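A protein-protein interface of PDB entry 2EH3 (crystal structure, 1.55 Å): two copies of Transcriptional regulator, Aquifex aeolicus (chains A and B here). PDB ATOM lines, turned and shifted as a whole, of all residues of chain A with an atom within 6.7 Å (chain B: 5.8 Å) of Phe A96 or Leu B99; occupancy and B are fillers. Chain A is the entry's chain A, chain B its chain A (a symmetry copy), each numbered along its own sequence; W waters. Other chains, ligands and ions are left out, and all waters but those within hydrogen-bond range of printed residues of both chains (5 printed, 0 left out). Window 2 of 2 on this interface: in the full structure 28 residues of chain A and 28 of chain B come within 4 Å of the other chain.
Phe A96 touches Leu B99, and with the chains exchanged Leu A99 touches Phe B96.
Cys A100 touches its own counterpart, Cys B100.
Phe A96 touches two residues of chain B.
Of chain A, only Phe A96 (3.4 Å) comes within 4 Å of Leu B99.
Of the printed residues of chain B, Leu A147 touches Tyr B108 and Phe B109.
Of the printed residues of chain A, Phe B96 touches Leu A99 (3.4 Å).
The nearest residue of chain A that does not touch Leu B99 is Leu A95 (4.2 Å).
O of Phe B94 sits at hydrogen-bond distance from N of Leu B99, at 3.1 Å.
The side-chain carboxylate of Glu B102 lies within salt-bridge range of the guanidinium group of Arg B105, at 3.6 Å.
O of Leu B98 is in hydrogen-bond range of N of Arg B105 (3.4 Å).
The backbone NH of Cys A100 sits at hydrogen-bond distance from the backbone carbonyl oxygen of Leu A95, at 3.1 Å.
The backbone carbonyl oxygen (O) of Ser B101 lies within hydrogen-bond range of the guanidinium group (NH2) of Arg B105, at 3.2 Å.
The guanidinium group (NE) of Arg B105 sits at hydrogen-bond distance from the backbone carbonyl oxygen (O) of Leu B99, 3.0 Å away.
SG of Cys B100 is disulfide-bonded to SG of Cys A100 (2.0 Å).
The guanidinium group (NH1) of Arg B105 lies within hydrogen-bond range of the side-chain hydroxyl (OH) of Tyr A92 (2.9 Å).
Phe A96 touches Leu B99 (CE1 to O, 3.4 Å).
NH2 of Arg B105 touches CE1 of Phe A96, 3.2 Å away.
Phe B96 touches Leu A99 (CE1 to O, 3.4 Å).
Tyr B108 touches Leu A147 (OH to CD2, 3.8 Å).
Phe B109 touches Leu A147 (CE1 to CG, 3.7 Å).
Of the 14 printed residues of chain B, 6 touch a printed residue of chain A.
Along chain B the printed residues that touch a printed residue of chain A span positions 96 to 109.
Of the 14 printed residues of chain A, 5 touch a printed residue of chain B.
Printed residues of chain A that touch a printed residue of chain B: Tyr A92, Phe A96, Leu A99, Cys A100 and Leu A147.
Hydrophobic or aromatic side chains of chain A within 4 Å of the printed part of chain B: Tyr A92, Phe A96 and Leu A147.
Water W5 lies within hydrogen-bond range of the side-chain carboxylate of Glu B102 (2.5 Å), the side-chain hydroxyl of Tyr A92 (2.8 Å) and the guanidinium group of Arg B105 (2.9 Å).
Water W2 lies within hydrogen-bond range of the side-chain carboxylate (OE1) of Glu B102 and the side-chain hydroxyl (OH) of Tyr A92.
Water W3 bridges O of Cys A100 (2.8 Å) and O of Phe B96 (2.9 Å).
Water W4 bridges the backbone carbonyl oxygen (O) of Cys B100 and the backbone carbonyl oxygen (O) of Phe A96.
Water W1 lies within hydrogen-bond range of the backbone carbonyl oxygen (O) of Ile A151 and the guanidinium group (NH1) of Arg B105.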
ATOM      1  N   TYR A  20      12.260  21.424 -30.799  1.00  0.00           N
ATOM      2  CA  TYR A  20      11.478  20.563 -31.684  1.00  0.00           C
ATOM      3  C   TYR A  20       9.966  20.791 -31.519  1.00  0.00           C
ATOM      4  O   TYR A  20       9.268  21.027 -32.502  1.00  0.00           O
ATOM      5  CB  TYR A  20      11.801  19.100 -31.377  1.00  0.00           C
ATOM      6  CG  TYR A  20      10.957  18.120 -32.145  1.00  0.00           C
ATOM      7  CD1 TYR A  20      11.304  17.740 -33.461  1.00  0.00           C
ATOM      8  CD2 TYR A  20       9.845  17.529 -31.555  1.00  0.00           C
ATOM      9  CE1 TYR A  20      10.566  16.781 -34.152  1.00  0.00           C
ATOM     10  CE2 TYR A  20       9.099  16.584 -32.242  1.00  0.00           C
ATOM     11  CZ  TYR A  20       9.466  16.211 -33.528  1.00  0.00           C
ATOM     12  OH  TYR A  20       8.740  15.233 -34.170  1.00  0.00           O
ATOM     13  N   VAL A  91      24.205  18.627 -31.009  1.00  0.00           N
ATOM     14  CA  VAL A  91      24.426  18.166 -29.651  1.00  0.00           C
ATOM     15  C   VAL A  91      23.383  18.819 -28.749  1.00  0.00           C
ATOM     16  O   VAL A  91      22.826  18.171 -27.872  1.00  0.00           O
ATOM     17  CB  VAL A  91      25.853  18.530 -29.158  1.00  0.00           C
ATOM     18  CG1 VAL A  91      25.973  18.237 -27.660  1.00  0.00           C
ATOM     19  CG2 VAL A  91      26.886  17.728 -29.947  1.00  0.00           C
ATOM     20  N   TYR A  92      23.105  20.103 -28.983  1.00  0.00           N
ATOM     21  CA  TYR A  92      22.115  20.829 -28.194  1.00  0.00           C
ATOM     22  C   TYR A  92      20.724  20.190 -28.403  1.00  0.00           C
ATOM     23  O   TYR A  92      19.984  19.931 -27.438  1.00  0.00           O
ATOM     24  CB  TYR A  92      22.163  22.301 -28.628  1.00  0.00           C
ATOM     25  CG  TYR A  92      21.382  23.235 -27.769  1.00  0.00           C
ATOM     26  CD1 TYR A  92      20.004  23.346 -27.930  1.00  0.00           C
ATOM     27  CD2 TYR A  92      22.009  24.007 -26.797  1.00  0.00           C
ATOM     28  CE1 TYR A  92      19.267  24.206 -27.140  1.00  0.00           C
ATOM     29  CE2 TYR A  92      21.289  24.867 -26.002  1.00  0.00           C
ATOM     30  CZ  TYR A  92      19.922  24.963 -26.175  1.00  0.00           C
ATOM     31  OH  TYR A  92      19.202  25.812 -25.374  1.00  0.00           O
ATOM     32  N   ILE A  93      20.365  19.893 -29.655  1.00  0.00           N
ATOM     33  CA  ILE A  93      19.074  19.261 -29.953  1.00  0.00           C
ATOM     34  C   ILE A  93      18.990  17.873 -29.285  1.00  0.00           C
ATOM     35  O   ILE A  93      17.967  17.482 -28.693  1.00  0.00           O
ATOM     36  CB  ILE A  93      18.919  19.155 -31.505  1.00  0.00           C
ATOM     37  CG1 ILE A  93      18.766  20.569 -32.090  1.00  0.00           C
ATOM     38  CG2 ILE A  93      17.701  18.280 -31.874  1.00  0.00           C
ATOM     39  CD1 ILE A  93      18.994  20.646 -33.637  1.00  0.00           C
ATOM     40  N   PHE A  94      20.083  17.120 -29.376  1.00  0.00           N
ATOM     41  CA  PHE A  94      20.173  15.801 -28.786  1.00  0.00           C
ATOM     42  C   PHE A  94      19.806  15.836 -27.287  1.00  0.00           C
ATOM     43  O   PHE A  94      19.039  15.006 -26.792  1.00  0.00           O
ATOM     44  CB  PHE A  94      21.621  15.327 -28.985  1.00  0.00           C
ATOM     45  CG  PHE A  94      21.873  13.881 -28.665  1.00  0.00           C
ATOM     46  CD1 PHE A  94      21.222  12.871 -29.351  1.00  0.00           C
ATOM     47  CD2 PHE A  94      22.825  13.546 -27.712  1.00  0.00           C
ATOM     48  CE1 PHE A  94      21.516  11.532 -29.097  1.00  0.00           C
ATOM     49  CE2 PHE A  94      23.129  12.206 -27.447  1.00  0.00           C
ATOM     50  CZ  PHE A  94      22.468  11.203 -28.146  1.00  0.00           C
ATOM     51  N   LEU A  95      20.367  16.795 -26.559  1.00  0.00           N
ATOM     52  CA  LEU A  95      20.020  16.900 -25.139  1.00  0.00           C
ATOM     53  C   LEU A  95      18.613  17.449 -24.865  1.00  0.00           C
ATOM     54  O   LEU A  95      17.772  16.788 -24.216  1.00  0.00           O
ATOM     55  CB  LEU A  95      21.059  17.792 -24.445  1.00  0.00           C
ATOM     56  CG  LEU A  95      20.804  18.199 -22.995  1.00  0.00           C
ATOM     57  CD1 LEU A  95      20.612  16.989 -22.107  1.00  0.00           C
ATOM     58  CD2 LEU A  95      21.983  19.048 -22.507  1.00  0.00           C
ATOM     59  N   PHE A  96      18.322  18.625 -25.406  1.00  0.00           N
ATOM     60  CA  PHE A  96      17.068  19.275 -25.060  1.00  0.00           C
ATOM     61  C   PHE A  96      15.821  18.803 -25.736  1.00  0.00           C
ATOM     62  O   PHE A  96      14.729  18.963 -25.182  1.00  0.00           O
ATOM     63  CB  PHE A  96      17.249  20.780 -25.199  1.00  0.00           C
ATOM     64  CG  PHE A  96      18.256  21.330 -24.238  1.00  0.00           C
ATOM     65  CD1 PHE A  96      18.025  21.259 -22.856  1.00  0.00           C
ATOM     66  CD2 PHE A  96      19.450  21.884 -24.687  1.00  0.00           C
ATOM     67  CE1 PHE A  96      18.967  21.738 -21.940  1.00  0.00           C
ATOM     68  CE2 PHE A  96      20.395  22.361 -23.771  1.00  0.00           C
ATOM     69  CZ  PHE A  96      20.155  22.291 -22.402  1.00  0.00           C
ATOM     70  N   ASP A  97      15.973  18.218 -26.923  1.00  0.00           N
ATOM     71  CA  ASP A  97      14.840  17.664 -27.640  1.00  0.00           C
ATOM     72  C   ASP A  97      14.700  16.136 -27.544  1.00  0.00           C
ATOM     73  O   ASP A  97      13.590  15.602 -27.765  1.00  0.00           O
ATOM     74  CB  ASP A  97      14.882  18.088 -29.101  1.00  0.00           C
ATOM     75  CG  ASP A  97      14.734  19.574 -29.260  1.00  0.00           C
ATOM     76  OD1 ASP A  97      13.760  20.142 -28.735  1.00  0.00           O
ATOM     77  OD2 ASP A  97      15.623  20.158 -29.905  1.00  0.00           O
ATOM     78  N   LEU A  98      15.781  15.416 -27.224  1.00  0.00           N
ATOM     79  CA  LEU A  98      15.659  13.973 -27.101  1.00  0.00           C
ATOM     80  C   LEU A  98      15.757  13.481 -25.661  1.00  0.00           C
ATOM     81  O   LEU A  98      14.805  12.868 -25.191  1.00  0.00           O
ATOM     82  CB  LEU A  98      16.653  13.242 -28.031  1.00  0.00           C
ATOM     83  CG  LEU A  98      16.288  13.295 -29.534  1.00  0.00           C
ATOM     84  CD1 LEU A  98      16.826  14.544 -30.190  1.00  0.00           C
ATOM     85  CD2 LEU A  98      16.869  12.047 -30.230  1.00  0.00           C
ATOM     86  N   LEU A  99      16.857  13.740 -24.954  1.00  0.00           N
ATOM     87  CA  LEU A  99      16.926  13.280 -23.562  1.00  0.00           C
ATOM     88  C   LEU A  99      15.774  13.860 -22.750  1.00  0.00           C
ATOM     89  O   LEU A  99      15.110  13.137 -21.994  1.00  0.00           O
ATOM     90  CB  LEU A  99      18.266  13.682 -22.924  1.00  0.00           C
ATOM     91  CG  LEU A  99      18.305  13.451 -21.397  1.00  0.00           C
ATOM     92  CD1 LEU A  99      18.141  11.954 -21.117  1.00  0.00           C
ATOM     93  CD2 LEU A  99      19.655  13.958 -20.795  1.00  0.00           C
ATOM     94  N   CYS A 100      15.520  15.151 -22.922  1.00  0.00           N
ATOM     95  CA  CYS A 100      14.484  15.842 -22.157  1.00  0.00           C
ATOM     96  C   CYS A 100      13.066  15.448 -22.517  1.00  0.00           C
ATOM     97  O   CYS A 100      12.130  15.712 -21.765  1.00  0.00           O
ATOM     98  CB  CYS A 100      14.691  17.354 -22.308  1.00  0.00           C
ATOM     99  SG  CYS A 100      16.212  17.942 -21.514  1.00  0.00           S
ATOM    100  N   SER A 101      12.903  14.769 -23.642  1.00  0.00           N
ATOM    101  CA  SER A 101      11.557  14.363 -24.069  1.00  0.00           C
ATOM    102  C   SER A 101      11.174  13.045 -23.450  1.00  0.00           C
ATOM    103  O   SER A 101      12.026  12.345 -22.921  1.00  0.00           O
ATOM    104  CB  SER A 101      11.548  14.182 -25.587  1.00  0.00           C
ATOM    105  OG  SER A 101      12.131  12.923 -25.919  1.00  0.00           O
ATOM    106  N   LEU A 147      28.709  19.789 -21.674  1.00  0.00           N
ATOM    107  CA  LEU A 147      27.601  20.401 -20.961  1.00  0.00           C
ATOM    108  C   LEU A 147      27.993  21.752 -20.354  1.00  0.00           C
ATOM    109  O   LEU A 147      27.249  22.732 -20.407  1.00  0.00           O
ATOM    110  CB  LEU A 147      27.128  19.446 -19.863  1.00  0.00           C
ATOM    111  CG  LEU A 147      25.909  19.901 -19.087  1.00  0.00           C
ATOM    112  CD1 LEU A 147      24.688  19.888 -19.994  1.00  0.00           C
ATOM    113  CD2 LEU A 147      25.708  18.957 -17.934  1.00  0.00           C
ATOM    114  N   ILE A 151      27.329  23.875 -23.769  1.00  0.00           N
ATOM    115  CA  ILE A 151      25.908  24.148 -23.475  1.00  0.00           C
ATOM    116  C   ILE A 151      25.632  25.288 -22.507  1.00  0.00           C
ATOM    117  O   ILE A 151      24.848  26.193 -22.818  1.00  0.00           O
ATOM    118  CB  ILE A 151      25.184  22.892 -22.919  1.00  0.00           C
ATOM    119  CG1 ILE A 151      25.288  21.751 -23.932  1.00  0.00           C
ATOM    120  CG2 ILE A 151      23.717  23.232 -22.582  1.00  0.00           C
ATOM    121  CD1 ILE A 151      24.723  22.088 -25.305  1.00  0.00           C
ATOM    122  N   ILE B  93      14.248  14.909 -10.783  1.00  0.00           N
ATOM    123  CA  ILE B  93      13.605  16.221 -10.933  1.00  0.00           C
ATOM    124  C   ILE B  93      14.639  17.276 -11.382  1.00  0.00           C
ATOM    125  O   ILE B  93      14.390  18.114 -12.268  1.00  0.00           O
ATOM    126  CB  ILE B  93      12.951  16.611  -9.569  1.00  0.00           C
ATOM    127  CG1 ILE B  93      11.769  15.666  -9.292  1.00  0.00           C
ATOM    128  CG2 ILE B  93      12.477  18.081  -9.591  1.00  0.00           C
ATOM    129  CD1 ILE B  93      11.274  15.683  -7.807  1.00  0.00           C
ATOM    130  N   PHE B  94      15.817  17.230 -10.765  1.00  0.00           N
ATOM    131  CA  PHE B  94      16.899  18.137 -11.084  1.00  0.00           C
ATOM    132  C   PHE B  94      17.211  18.121 -12.596  1.00  0.00           C
ATOM    133  O   PHE B  94      17.365  19.168 -13.233  1.00  0.00           O
ATOM    134  CB  PHE B  94      18.117  17.675 -10.268  1.00  0.00           C
ATOM    135  CG  PHE B  94      19.281  18.622 -10.261  1.00  0.00           C
ATOM    136  CD1 PHE B  94      19.160  19.905  -9.753  1.00  0.00           C
ATOM    137  CD2 PHE B  94      20.522  18.187 -10.706  1.00  0.00           C
ATOM    138  CE1 PHE B  94      20.265  20.751  -9.683  1.00  0.00           C
ATOM    139  CE2 PHE B  94      21.639  19.027 -10.643  1.00  0.00           C
ATOM    140  CZ  PHE B  94      21.501  20.311 -10.129  1.00  0.00           C
ATOM    141  N   LEU B  95      17.316  16.929 -13.169  1.00  0.00           N
ATOM    142  CA  LEU B  95      17.569  16.856 -14.611  1.00  0.00           C
ATOM    143  C   LEU B  95      16.365  17.225 -15.489  1.00  0.00           C
ATOM    144  O   LEU B  95      16.427  18.160 -16.318  1.00  0.00           O
ATOM    145  CB  LEU B  95      18.036  15.436 -14.957  1.00  0.00           C
ATOM    146  CG  LEU B  95      18.185  15.066 -16.432  1.00  0.00           C
ATOM    147  CD1 LEU B  95      19.122  16.014 -17.147  1.00  0.00           C
ATOM    148  CD2 LEU B  95      18.693  13.623 -16.529  1.00  0.00           C
ATOM    149  N   PHE B  96      15.247  16.544 -15.274  1.00  0.00           N
ATOM    150  CA  PHE B  96      14.118  16.732 -16.172  1.00  0.00           C
ATOM    151  C   PHE B  96      13.262  17.943 -15.982  1.00  0.00           C
ATOM    152  O   PHE B  96      12.621  18.393 -16.937  1.00  0.00           O
ATOM    153  CB  PHE B  96      13.291  15.454 -16.182  1.00  0.00           C
ATOM    154  CG  PHE B  96      14.045  14.285 -16.736  1.00  0.00           C
ATOM    155  CD1 PHE B  96      14.468  14.288 -18.073  1.00  0.00           C
ATOM    156  CD2 PHE B  96      14.372  13.196 -15.934  1.00  0.00           C
ATOM    157  CE1 PHE B  96      15.202  13.221 -18.601  1.00  0.00           C
ATOM    158  CE2 PHE B  96      15.108  12.129 -16.462  1.00  0.00           C
ATOM    159  CZ  PHE B  96      15.520  12.138 -17.791  1.00  0.00           C
ATOM    160  N   ASP B  97      13.252  18.478 -14.762  1.00  0.00           N
ATOM    161  CA  ASP B  97      12.508  19.692 -14.480  1.00  0.00           C
ATOM    162  C   ASP B  97      13.360  20.969 -14.411  1.00  0.00           C
ATOM    163  O   ASP B  97      12.816  22.085 -14.572  1.00  0.00           O
ATOM    164  CB  ASP B  97      11.710  19.534 -13.193  1.00  0.00           C
ATOM    165  CG  ASP B  97      10.656  18.470 -13.312  1.00  0.00           C
ATOM    166  OD1 ASP B  97       9.843  18.531 -14.250  1.00  0.00           O
ATOM    167  OD2 ASP B  97      10.676  17.567 -12.457  1.00  0.00           O
ATOM    168  N   LEU B  98      14.672  20.849 -14.177  1.00  0.00           N
ATOM    169  CA  LEU B  98      15.496  22.045 -14.138  1.00  0.00           C
ATOM    170  C   LEU B  98      16.425  22.176 -15.340  1.00  0.00           C
ATOM    171  O   LEU B  98      16.311  23.163 -16.057  1.00  0.00           O
ATOM    172  CB  LEU B  98      16.263  22.157 -12.800  1.00  0.00           C
ATOM    173  CG  LEU B  98      15.385  22.541 -11.584  1.00  0.00           C
ATOM    174  CD1 LEU B  98      14.758  21.323 -10.950  1.00  0.00           C
ATOM    175  CD2 LEU B  98      16.264  23.276 -10.551  1.00  0.00           C
ATOM    176  N   LEU B  99      17.318  21.217 -15.586  1.00  0.00           N
ATOM    177  CA  LEU B  99      18.187  21.347 -16.761  1.00  0.00           C
ATOM    178  C   LEU B  99      17.355  21.464 -18.032  1.00  0.00           C
ATOM    179  O   LEU B  99      17.619  22.328 -18.881  1.00  0.00           O
ATOM    180  CB  LEU B  99      19.135  20.141 -16.870  1.00  0.00           C
ATOM    181  CG  LEU B  99      19.901  20.089 -18.210  1.00  0.00           C
ATOM    182  CD1 LEU B  99      20.790  21.331 -18.322  1.00  0.00           C
ATOM    183  CD2 LEU B  99      20.778  18.799 -18.297  1.00  0.00           C
ATOM    184  N   CYS B 100      16.339  20.620 -18.154  1.00  0.00           N
ATOM    185  CA  CYS B 100      15.502  20.587 -19.352  1.00  0.00           C
ATOM    186  C   CYS B 100      14.605  21.794 -19.528  1.00  0.00           C
ATOM    187  O   CYS B 100      14.088  22.041 -20.616  1.00  0.00           O
ATOM    188  CB  CYS B 100      14.685  19.289 -19.342  1.00  0.00           C
ATOM    189  SG  CYS B 100      15.709  17.806 -19.547  1.00  0.00           S
ATOM    190  N   SER B 101      14.454  22.583 -18.476  1.00  0.00           N
ATOM    191  CA  SER B 101      13.588  23.767 -18.560  1.00  0.00           C
ATOM    192  C   SER B 101      14.351  24.951 -19.091  1.00  0.00           C
ATOM    193  O   SER B 101      15.572  24.923 -19.140  1.00  0.00           O
ATOM    194  CB  SER B 101      13.092  24.125 -17.158  1.00  0.00           C
ATOM    195  OG  SER B 101      14.122  24.818 -16.454  1.00  0.00           O
ATOM    196  N   GLU B 102      13.659  25.994 -19.549  1.00  0.00           N
ATOM    197  CA  GLU B 102      14.410  27.181 -19.913  1.00  0.00           C
ATOM    198  C   GLU B 102      14.508  28.060 -18.652  1.00  0.00           C
ATOM    199  O   GLU B 102      15.570  28.616 -18.340  1.00  0.00           O
ATOM    200  CB  GLU B 102      13.699  27.985 -21.016  1.00  0.00           C
ATOM    201  CG  GLU B 102      13.681  27.313 -22.349  1.00  0.00           C
ATOM    202  CD  GLU B 102      15.041  27.284 -23.013  1.00  0.00           C
ATOM    203  OE1 GLU B 102      15.966  28.027 -22.594  1.00  0.00           O
ATOM    204  OE2 GLU B 102      15.179  26.523 -23.993  1.00  0.00           O
ATOM    205  N   PHE B 104      14.407  27.349 -15.361  1.00  0.00           N
ATOM    206  CA  PHE B 104      15.209  26.905 -14.219  1.00  0.00           C
ATOM    207  C   PHE B 104      16.590  26.356 -14.568  1.00  0.00           C
ATOM    208  O   PHE B 104      17.305  25.879 -13.682  1.00  0.00           O
ATOM    209  CB  PHE B 104      14.430  25.833 -13.422  1.00  0.00           C
ATOM    210  CG  PHE B 104      13.074  26.282 -12.944  1.00  0.00           C
ATOM    211  CD1 PHE B 104      12.925  27.472 -12.237  1.00  0.00           C
ATOM    212  CD2 PHE B 104      11.964  25.481 -13.148  1.00  0.00           C
ATOM    213  CE1 PHE B 104      11.676  27.848 -11.731  1.00  0.00           C
ATOM    214  CE2 PHE B 104      10.698  25.853 -12.637  1.00  0.00           C
ATOM    215  CZ  PHE B 104      10.565  27.034 -11.931  1.00  0.00           C
ATOM    216  N   ARG B 105      16.989  26.445 -15.833  1.00  0.00           N
ATOM    217  CA  ARG B 105      18.308  25.937 -16.235  1.00  0.00           C
ATOM    218  C   ARG B 105      19.453  26.523 -15.426  1.00  0.00           C
ATOM    219  O   ARG B 105      20.407  25.808 -15.082  1.00  0.00           O
ATOM    220  CB  ARG B 105      18.560  26.210 -17.721  1.00  0.00           C
ATOM    221  CG  ARG B 105      19.765  25.416 -18.263  1.00  0.00           C
ATOM    222  CD  ARG B 105      19.792  25.424 -19.786  1.00  0.00           C
ATOM    223  NE  ARG B 105      18.560  24.834 -20.293  1.00  0.00           N
ATOM    224  CZ  ARG B 105      18.170  24.855 -21.561  1.00  0.00           C
ATOM    225  NH1 ARG B 105      18.932  25.441 -22.479  1.00  0.00           N
ATOM    226  NH2 ARG B 105      17.016  24.298 -21.905  1.00  0.00           N
ATOM    227  N   TYR B 108      20.105  24.639 -12.125  1.00  0.00           N
ATOM    228  CA  TYR B 108      20.784  23.371 -12.348  1.00  0.00           C
ATOM    229  C   TYR B 108      22.265  23.663 -12.405  1.00  0.00           C
ATOM    230  O   TYR B 108      23.056  23.070 -11.667  1.00  0.00           O
ATOM    231  CB  TYR B 108      20.353  22.757 -13.681  1.00  0.00           C
ATOM    232  CG  TYR B 108      21.109  21.517 -14.078  1.00  0.00           C
ATOM    233  CD1 TYR B 108      20.719  20.254 -13.617  1.00  0.00           C
ATOM    234  CD2 TYR B 108      22.197  21.592 -14.939  1.00  0.00           C
ATOM    235  CE1 TYR B 108      21.393  19.100 -14.019  1.00  0.00           C
ATOM    236  CE2 TYR B 108      22.887  20.454 -15.345  1.00  0.00           C
ATOM    237  CZ  TYR B 108      22.475  19.200 -14.884  1.00  0.00           C
ATOM    238  OH  TYR B 108      23.146  18.082 -15.334  1.00  0.00           O
ATOM    239  N   PHE B 109      22.652  24.594 -13.266  1.00  0.00           N
ATOM    240  CA  PHE B 109      24.085  24.890 -13.354  1.00  0.00           C
ATOM    241  C   PHE B 109      24.689  25.534 -12.111  1.00  0.00           C
ATOM    242  O   PHE B 109      25.870  25.285 -11.792  1.00  0.00           O
ATOM    243  CB  PHE B 109      24.382  25.707 -14.619  1.00  0.00           C
ATOM    244  CG  PHE B 109      24.320  24.883 -15.878  1.00  0.00           C
ATOM    245  CD1 PHE B 109      25.174  23.786 -16.040  1.00  0.00           C
ATOM    246  CD2 PHE B 109      23.379  25.158 -16.877  1.00  0.00           C
ATOM    247  CE1 PHE B 109      25.096  22.965 -17.177  1.00  0.00           C
ATOM    248  CE2 PHE B 109      23.293  24.337 -18.032  1.00  0.00           C
ATOM    249  CZ  PHE B 109      24.152  23.237 -18.174  1.00  0.00           C
HETATM  250  O   HOH W   1      22.023  26.440 -22.152  1.00  0.00           O
HETATM  251  O   HOH W   2      18.022  28.542 -24.200  1.00  0.00           O
HETATM  252  O   HOH W   3      11.753  16.824 -19.178  1.00  0.00           O
HETATM  253  O   HOH W   4      14.178  21.030 -23.269  1.00  0.00           O
HETATM  254  O   HOH W   5      16.727  24.680 -24.781  1.00  0.00           O
